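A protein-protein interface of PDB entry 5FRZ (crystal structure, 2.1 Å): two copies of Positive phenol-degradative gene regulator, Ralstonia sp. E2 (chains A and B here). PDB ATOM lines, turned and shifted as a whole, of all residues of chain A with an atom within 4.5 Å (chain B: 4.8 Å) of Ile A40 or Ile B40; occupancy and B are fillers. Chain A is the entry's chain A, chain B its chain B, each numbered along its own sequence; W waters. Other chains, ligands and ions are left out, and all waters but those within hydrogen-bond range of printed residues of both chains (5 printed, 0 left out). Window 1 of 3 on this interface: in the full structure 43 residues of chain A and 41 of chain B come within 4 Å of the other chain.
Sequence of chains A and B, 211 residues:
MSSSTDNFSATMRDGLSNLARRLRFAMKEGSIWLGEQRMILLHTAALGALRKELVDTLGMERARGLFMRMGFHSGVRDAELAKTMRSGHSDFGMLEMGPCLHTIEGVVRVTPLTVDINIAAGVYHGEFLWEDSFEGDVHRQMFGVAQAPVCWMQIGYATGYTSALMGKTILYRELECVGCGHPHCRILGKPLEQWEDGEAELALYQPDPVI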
ATOM      1  N   MET A  39      14.566  15.845 -24.726  1.00  0.00           N
ATOM      2  CA  MET A  39      15.459  14.830 -25.297  1.00  0.00           C
ATOM      3  C   MET A  39      16.866  14.951 -24.725  1.00  0.00           C
ATOM      4  O   MET A  39      17.245  16.018 -24.246  1.00  0.00           O
ATOM      5  CB  MET A  39      15.545  14.984 -26.829  1.00  0.00           C
ATOM      6  CG  MET A  39      14.207  15.275 -27.521  1.00  0.00           C
ATOM      7  SD  MET A  39      13.123  13.833 -27.685  1.00  0.00           S
ATOM      8  CE  MET A  39      14.042  12.854 -28.855  1.00  0.00           C
ATOM      9  N   ILE A  40      17.650  13.877 -24.806  1.00  0.00           N
ATOM     10  CA  ILE A  40      19.093  14.010 -24.663  1.00  0.00           C
ATOM     11  C   ILE A  40      19.808  13.434 -25.879  1.00  0.00           C
ATOM     12  O   ILE A  40      19.278  12.568 -26.600  1.00  0.00           O
ATOM     13  CB  ILE A  40      19.649  13.324 -23.391  1.00  0.00           C
ATOM     14  CG1 ILE A  40      19.387  11.827 -23.403  1.00  0.00           C
ATOM     15  CG2 ILE A  40      19.117  13.996 -22.120  1.00  0.00           C
ATOM     16  CD1 ILE A  40      19.992  11.136 -22.225  1.00  0.00           C
ATOM     17  N   LEU A  41      21.012  13.944 -26.112  1.00  0.00           N
ATOM     18  CA  LEU A  41      21.942  13.310 -27.036  1.00  0.00           C
ATOM     19  C   LEU A  41      22.713  12.277 -26.262  1.00  0.00           C
ATOM     20  O   LEU A  41      23.391  12.598 -25.275  1.00  0.00           O
ATOM     21  CB  LEU A  41      22.890  14.330 -27.664  1.00  0.00           C
ATOM     22  CG  LEU A  41      22.261  15.215 -28.720  1.00  0.00           C
ATOM     23  CD1 LEU A  41      23.039  16.511 -28.849  1.00  0.00           C
ATOM     24  CD2 LEU A  41      22.222  14.459 -30.048  1.00  0.00           C
ATOM     25  N   LEU A  42      22.629  11.033 -26.712  1.00  0.00           N
ATOM     26  CA  LEU A  42      23.311   9.960 -26.017  1.00  0.00           C
ATOM     27  C   LEU A  42      24.278   9.227 -26.941  1.00  0.00           C
ATOM     28  O   LEU A  42      23.913   8.867 -28.055  1.00  0.00           O
ATOM     29  CB  LEU A  42      22.301   8.981 -25.441  1.00  0.00           C
ATOM     30  CG  LEU A  42      22.869   7.845 -24.600  1.00  0.00           C
ATOM     31  CD1 LEU A  42      23.605   8.372 -23.410  1.00  0.00           C
ATOM     32  CD2 LEU A  42      21.707   6.957 -24.158  1.00  0.00           C
ATOM     33  N   THR A  44      26.001   6.390 -28.758  1.00  0.00           N
ATOM     34  CA  THR A  44      25.558   5.026 -29.044  1.00  0.00           C
ATOM     35  C   THR A  44      26.464   4.012 -28.355  1.00  0.00           C
ATOM     36  O   THR A  44      26.043   2.891 -28.076  1.00  0.00           O
ATOM     37  CB  THR A  44      25.518   4.727 -30.561  1.00  0.00           C
ATOM     38  OG1 THR A  44      26.800   5.001 -31.128  1.00  0.00           O
ATOM     39  CG2 THR A  44      24.474   5.598 -31.249  1.00  0.00           C
ATOM     40  N   LEU A  47      25.034   3.497 -24.924  1.00  0.00           N
ATOM     41  CA  LEU A  47      23.896   2.575 -25.008  1.00  0.00           C
ATOM     42  C   LEU A  47      24.397   1.149 -25.228  1.00  0.00           C
ATOM     43  O   LEU A  47      23.846   0.200 -24.682  1.00  0.00           O
ATOM     44  CB  LEU A  47      22.948   2.956 -26.142  1.00  0.00           C
ATOM     45  CG  LEU A  47      21.655   3.716 -25.829  1.00  0.00           C
ATOM     46  CD1 LEU A  47      20.756   3.731 -27.041  1.00  0.00           C
ATOM     47  CD2 LEU A  47      20.923   3.173 -24.607  1.00  0.00           C
ATOM     48  N   GLU A 105      16.404  11.959 -35.340  1.00  0.00           N
ATOM     49  CA  GLU A 105      16.948  11.504 -34.065  1.00  0.00           C
ATOM     50  C   GLU A 105      18.235  10.692 -34.228  1.00  0.00           C
ATOM     51  O   GLU A 105      18.773  10.206 -33.237  1.00  0.00           O
ATOM     52  CB  GLU A 105      15.889  10.687 -33.294  1.00  0.00           C
ATOM     53  CG  GLU A 105      14.704  11.549 -32.813  1.00  0.00           C
ATOM     54  CD  GLU A 105      13.442  10.768 -32.505  1.00  0.00           C
ATOM     55  OE1 GLU A 105      13.463   9.502 -32.450  1.00  0.00           O
ATOM     56  OE2 GLU A 105      12.400  11.451 -32.329  1.00  0.00           O
ATOM     57  N   GLY A 106      18.730  10.564 -35.464  1.00  0.00           N
ATOM     58  CA  GLY A 106      20.003   9.898 -35.728  1.00  0.00           C
ATOM     59  C   GLY A 106      20.007   8.382 -35.560  1.00  0.00           C
ATOM     60  O   GLY A 106      21.053   7.739 -35.395  1.00  0.00           O
ATOM     61  N   VAL A 107      18.824   7.798 -35.595  1.00  0.00           N
ATOM     62  CA  VAL A 107      18.690   6.366 -35.351  1.00  0.00           C
ATOM     63  C   VAL A 107      18.963   5.534 -36.621  1.00  0.00           C
ATOM     64  O   VAL A 107      19.668   4.530 -36.577  1.00  0.00           O
ATOM     65  CB  VAL A 107      17.266   6.060 -34.774  1.00  0.00           C
ATOM     66  CG1 VAL A 107      16.945   4.552 -34.818  1.00  0.00           C
ATOM     67  CG2 VAL A 107      17.142   6.625 -33.344  1.00  0.00           C
ATOM     68  N   PHE A 134      21.740   2.625 -36.379  1.00  0.00           N
ATOM     69  CA  PHE A 134      22.691   2.808 -35.290  1.00  0.00           C
ATOM     70  C   PHE A 134      22.762   1.523 -34.501  1.00  0.00           C
ATOM     71  O   PHE A 134      23.833   1.106 -34.084  1.00  0.00           O
ATOM     72  CB  PHE A 134      22.305   3.974 -34.367  1.00  0.00           C
ATOM     73  CG  PHE A 134      21.525   3.552 -33.144  1.00  0.00           C
ATOM     74  CD1 PHE A 134      22.184   3.119 -31.990  1.00  0.00           C
ATOM     75  CD2 PHE A 134      20.139   3.584 -33.148  1.00  0.00           C
ATOM     76  CE1 PHE A 134      21.480   2.701 -30.888  1.00  0.00           C
ATOM     77  CE2 PHE A 134      19.421   3.184 -32.041  1.00  0.00           C
ATOM     78  CZ  PHE A 134      20.094   2.742 -30.902  1.00  0.00           C
ATOM     79  N   ARG B  38      29.116   8.694 -32.717  1.00  0.00           N
ATOM     80  CA  ARG B  38      27.740   8.705 -33.197  1.00  0.00           C
ATOM     81  C   ARG B  38      26.782   8.862 -32.010  1.00  0.00           C
ATOM     82  O   ARG B  38      26.930   8.201 -30.990  1.00  0.00           O
ATOM     83  CB  ARG B  38      27.428   7.424 -33.993  1.00  0.00           C
ATOM     84  CG  ARG B  38      26.188   7.557 -34.822  1.00  0.00           C
ATOM     85  CD  ARG B  38      25.800   6.284 -35.570  1.00  0.00           C
ATOM     86  NE  ARG B  38      24.470   6.458 -36.138  1.00  0.00           N
ATOM     87  CZ  ARG B  38      23.902   5.642 -37.020  1.00  0.00           C
ATOM     88  NH1 ARG B  38      24.547   4.563 -37.457  1.00  0.00           N
ATOM     89  NH2 ARG B  38      22.678   5.910 -37.455  1.00  0.00           N
ATOM     90  N   MET B  39      25.814   9.754 -32.160  1.00  0.00           N
ATOM     91  CA  MET B  39      24.853  10.093 -31.115  1.00  0.00           C
ATOM     92  C   MET B  39      23.423   9.827 -31.587  1.00  0.00           C
ATOM     93  O   MET B  39      23.128   9.921 -32.785  1.00  0.00           O
ATOM     94  CB  MET B  39      24.975  11.571 -30.721  1.00  0.00           C
ATOM     95  CG  MET B  39      26.407  12.092 -30.534  1.00  0.00           C
ATOM     96  SD  MET B  39      27.212  11.413 -29.066  1.00  0.00           S
ATOM     97  CE  MET B  39      26.396  12.363 -27.771  1.00  0.00           C
ATOM     98  N   ILE B  40      22.528   9.531 -30.651  1.00  0.00           N
ATOM     99  CA  ILE B  40      21.100   9.565 -30.969  1.00  0.00           C
ATOM    100  C   ILE B  40      20.397  10.561 -30.051  1.00  0.00           C
ATOM    101  O   ILE B  40      20.811  10.760 -28.910  1.00  0.00           O
ATOM    102  CB  ILE B  40      20.419   8.174 -30.829  1.00  0.00           C
ATOM    103  CG1 ILE B  40      20.543   7.639 -29.397  1.00  0.00           C
ATOM    104  CG2 ILE B  40      21.003   7.179 -31.821  1.00  0.00           C
ATOM    105  CD1 ILE B  40      19.617   6.453 -29.122  1.00  0.00           C
ATOM    106  N   LEU B  41      19.349  11.199 -30.560  1.00  0.00           N
ATOM    107  CA  LEU B  41      18.448  11.957 -29.709  1.00  0.00           C
ATOM    108  C   LEU B  41      17.473  10.976 -29.115  1.00  0.00           C
ATOM    109  O   LEU B  41      16.762  10.283 -29.840  1.00  0.00           O
ATOM    110  CB  LEU B  41      17.710  13.041 -30.490  1.00  0.00           C
ATOM    111  CG  LEU B  41      18.477  14.334 -30.727  1.00  0.00           C
ATOM    112  CD1 LEU B  41      17.734  15.205 -31.733  1.00  0.00           C
ATOM    113  CD2 LEU B  41      18.684  15.070 -29.383  1.00  0.00           C
ATOM    114  N   LEU B  42      17.439  10.908 -27.792  1.00  0.00           N
ATOM    115  CA  LEU B  42      16.527   9.990 -27.129  1.00  0.00           C
ATOM    116  C   LEU B  42      15.583  10.718 -26.173  1.00  0.00           C
ATOM    117  O   LEU B  42      15.989  11.636 -25.449  1.00  0.00           O
ATOM    118  CB  LEU B  42      17.314   8.915 -26.383  1.00  0.00           C
ATOM    119  CG  LEU B  42      16.579   7.811 -25.629  1.00  0.00           C
ATOM    120  CD1 LEU B  42      15.712   7.006 -26.557  1.00  0.00           C
ATOM    121  CD2 LEU B  42      17.641   6.928 -24.962  1.00  0.00           C
ATOM    122  N   THR B  44      13.693  11.557 -22.955  1.00  0.00           N
ATOM    123  CA  THR B  44      13.962  11.273 -21.552  1.00  0.00           C
ATOM    124  C   THR B  44      12.865  10.416 -20.931  1.00  0.00           C
ATOM    125  O   THR B  44      13.130   9.627 -20.023  1.00  0.00           O
ATOM    126  CB  THR B  44      14.123  12.571 -20.753  1.00  0.00           C
ATOM    127  OG1 THR B  44      12.946  13.367 -20.913  1.00  0.00           O
ATOM    128  CG2 THR B  44      15.323  13.358 -21.281  1.00  0.00           C
ATOM    129  N   LEU B  47      13.849   6.845 -21.700  1.00  0.00           N
ATOM    130  CA  LEU B  47      14.921   6.462 -20.791  1.00  0.00           C
ATOM    131  C   LEU B  47      14.358   6.291 -19.378  1.00  0.00           C
ATOM    132  O   LEU B  47      14.761   5.402 -18.632  1.00  0.00           O
ATOM    133  CB  LEU B  47      16.029   7.511 -20.799  1.00  0.00           C
ATOM    134  CG  LEU B  47      17.216   7.333 -19.860  1.00  0.00           C
ATOM    135  CD1 LEU B  47      17.961   6.058 -20.237  1.00  0.00           C
ATOM    136  CD2 LEU B  47      18.160   8.548 -19.850  1.00  0.00           C
ATOM    137  N   GLU B 105      24.578  18.355 -24.725  1.00  0.00           N
ATOM    138  CA  GLU B 105      23.839  17.118 -24.894  1.00  0.00           C
ATOM    139  C   GLU B 105      22.449  17.155 -24.244  1.00  0.00           C
ATOM    140  O   GLU B 105      21.721  16.159 -24.289  1.00  0.00           O
ATOM    141  CB  GLU B 105      24.678  15.951 -24.359  1.00  0.00           C
ATOM    142  CG  GLU B 105      25.899  15.649 -25.277  1.00  0.00           C
ATOM    143  CD  GLU B 105      27.086  14.978 -24.542  1.00  0.00           C
ATOM    144  OE1 GLU B 105      26.908  14.436 -23.423  1.00  0.00           O
ATOM    145  OE2 GLU B 105      28.211  15.002 -25.094  1.00  0.00           O
ATOM    146  N   GLY B 106      22.089  18.308 -23.670  1.00  0.00           N
ATOM    147  CA  GLY B 106      20.803  18.518 -23.026  1.00  0.00           C
ATOM    148  C   GLY B 106      20.587  17.758 -21.732  1.00  0.00           C
ATOM    149  O   GLY B 106      19.461  17.633 -21.248  1.00  0.00           O
ATOM    150  N   VAL B 107      21.669  17.257 -21.154  1.00  0.00           N
ATOM    151  CA  VAL B 107      21.574  16.417 -19.973  1.00  0.00           C
ATOM    152  C   VAL B 107      21.270  17.249 -18.722  1.00  0.00           C
ATOM    153  O   VAL B 107      20.391  16.894 -17.937  1.00  0.00           O
ATOM    154  CB  VAL B 107      22.878  15.585 -19.774  1.00  0.00           C
ATOM    155  CG1 VAL B 107      22.909  14.930 -18.403  1.00  0.00           C
ATOM    156  CG2 VAL B 107      23.009  14.496 -20.881  1.00  0.00           C
ATOM    157  N   PHE B 134      18.229  16.279 -16.070  1.00  0.00           N
ATOM    158  CA  PHE B 134      17.143  15.511 -16.692  1.00  0.00           C
ATOM    159  C   PHE B 134      16.885  14.280 -15.832  1.00  0.00           C
ATOM    160  O   PHE B 134      15.752  13.870 -15.670  1.00  0.00           O
ATOM    161  CB  PHE B 134      17.453  15.110 -18.147  1.00  0.00           C
ATOM    162  CG  PHE B 134      18.032  13.736 -18.285  1.00  0.00           C
ATOM    163  CD1 PHE B 134      19.399  13.543 -18.223  1.00  0.00           C
ATOM    164  CD2 PHE B 134      17.206  12.630 -18.468  1.00  0.00           C
ATOM    165  CE1 PHE B 134      19.945  12.269 -18.328  1.00  0.00           C
ATOM    166  CE2 PHE B 134      17.748  11.346 -18.579  1.00  0.00           C
ATOM    167  CZ  PHE B 134      19.124  11.172 -18.514  1.00  0.00           C
HETATM  168  O   HOH W   1      25.072  12.193 -23.051  1.00  0.00           O
HETATM  169  O   HOH W   2      23.313   8.830 -35.159  1.00  0.00           O
HETATM  170  O   HOH W   3      29.169   6.967 -29.542  1.00  0.00           O
HETATM  171  O   HOH W   4      14.955   8.140 -30.650  1.00  0.00           O
HETATM  172  O   HOH W   5      17.308  17.948 -22.756  1.00  0.00           O
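NH2 of Arg B38 is in hydrogen-bond range of O of Val A107 (3.4 Å).
The backbone NH (N) of Leu B41 lies within hydrogen-bond range of the backbone carbonyl oxygen (O) of Glu A105 (2.9 Å).
The backbone carbonyl oxygen (O) of Ile A40 sits at hydrogen-bond distance from the backbone NH (N) of Leu B42 (2.7 Å).
The backbone NH (N) of Thr A44 is in hydrogen-bond range of the backbone carbonyl oxygen (O) of Arg B38, 3.0 Å away.
The backbone carbonyl oxygen (O) of Ile B40 is in hydrogen-bond range of the backbone NH (N) of Leu A42 (2.9 Å).
The backbone carbonyl oxygen of Ile A40 lies close to the backbone carbonyl oxygen of Ile B40 (3.3 Å).
NH2 of Arg B38 is in hydrogen-bond range of O of Gly A106 (3.2 Å).
The backbone NH of Leu A41 lies within hydrogen-bond range of the backbone carbonyl oxygen of Glu B105 (3.0 Å).
The backbone carbonyl oxygen of Val A107 lies within hydrogen-bond range of the backbone NH of Phe A134 (2.8 Å).
The backbone NH (N) of Phe B134 lies within hydrogen-bond range of the backbone carbonyl oxygen (O) of Val B107, at 2.9 Å.
Among the printed residues, merely in contact across the chains: Met A39 with Leu B42 (3.2 Å), Ile A40 with Leu B41 (3.3 Å), Glu A105 with Ile B40 (3.3 Å), Phe A134 with Arg B38 (3.3 Å), Leu A41 with Ile B40 (3.4 Å), Ile A40 with Glu B105 (3.4 Å), Leu A42 with Met B39 (3.4 Å), Leu A47 with Ile B40 (3.6 Å), Gly A106 with Ile B40 (3.6 Å), Leu A41 with Leu B41 (3.6 Å), Ile A40 with Gly B106 (3.8 Å), Ile A40 with Phe B134 (3.8 Å), Thr A44 with Ile B40 (3.9 Å), Met A39 with Leu B41 (3.9 Å), Phe A134 with Ile B40 (3.9 Å), Leu A41 with Met B39 (3.9 Å), Ile A40 with Thr B44 (3.9 Å), Ile A40 with Leu B47 (3.96 Å) and Gly A106 with Met B39 (3.98 Å).
Of the printed residues of chain B, Met A39 touches Leu B41 and Leu B42.
Of the printed residues of chain B, Ile A40 touches Ile B40, Leu B41, Leu B42, Thr B44, Leu B47, Glu B105, Gly B106 and Phe B134.
Printed residues of chain B within 4 Å of Leu A41: Met B39, Ile B40, Leu B41 and Glu B105.
Of the printed residues of chain B, Phe A134 touches Arg B38 (3.3 Å) and Ile B40 (3.9 Å).
Ile B40 touches just these residues of chain A: Ile A40 (3.3 Å), Leu A41 (3.4 Å), Leu A42 (2.9 Å), Thr A44 (3.9 Å), Leu A47 (3.6 Å), Glu A105 (3.3 Å), Gly A106 (3.6 Å) and Phe A134 (3.9 Å).
Of the printed residues of chain A, Phe B134 touches Ile A40.
The nearest residue of chain B that does not touch Ile A40 is Val B107 (4.1 Å).
The nearest printed residue of chain A that does not touch Phe B134 is Met A39 (6.2 Å).
Of the 10 printed residues of chain A, 10 touch a printed residue of chain B.
Printed residues of chain A that touch a printed residue of chain B: Met A39, Ile A40, Leu A41, Leu A42, Thr A44, Leu A47, Glu A105, Gly A106, Val A107 and Phe A134.
Of the 11 printed residues of chain B, 10 touch a printed residue of chain A.
Among the printed residues, 27 pairs touch across the chains.
Among the printed residues, no Asp or Glu carboxylate lies within 4 Å of a Lys or Arg side-chain nitrogen of the other chain.
Ile A40 touches Leu B41, and with the chains exchanged Leu A41 touches Ile B40.
Ile A40 touches Leu B47, and with the chains exchanged Leu A47 touches Ile B40.
Ile A40 touches Phe B134, and with the chains exchanged Phe A134 touches Ile B40.
Gly A106 touches Met B39, but with the chains exchanged Met A39 does not touch Gly B106 (4.1 Å).
Positions printed for both chains: 39, 40, 41, 42, 44, 47, 105, 106, 107 and 134.
Of the 27 pairs that touch across the chains among the printed residues, 22 have their exchanged pair printed and touching as well.
Water W5 bridges O of Met A39 and O of Gly B106.
Water W2 lies within hydrogen-bond range of the backbone carbonyl oxygen (O) of Gly A106 (2.5 Å), the backbone carbonyl oxygen (O) of Met B39 (2.6 Å) and the guanidinium group (NE) of Arg B38 (2.8 Å).
Water W4 lies within hydrogen-bond range of the side-chain carboxylate of Glu A105 and the backbone carbonyl oxygen of Leu B41.
Water W1 bridges O of Leu A41 and OE1 of Glu B105.
Water W3 bridges O of Arg B38 (2.9 Å) and N of Thr A44 (3.3 Å).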
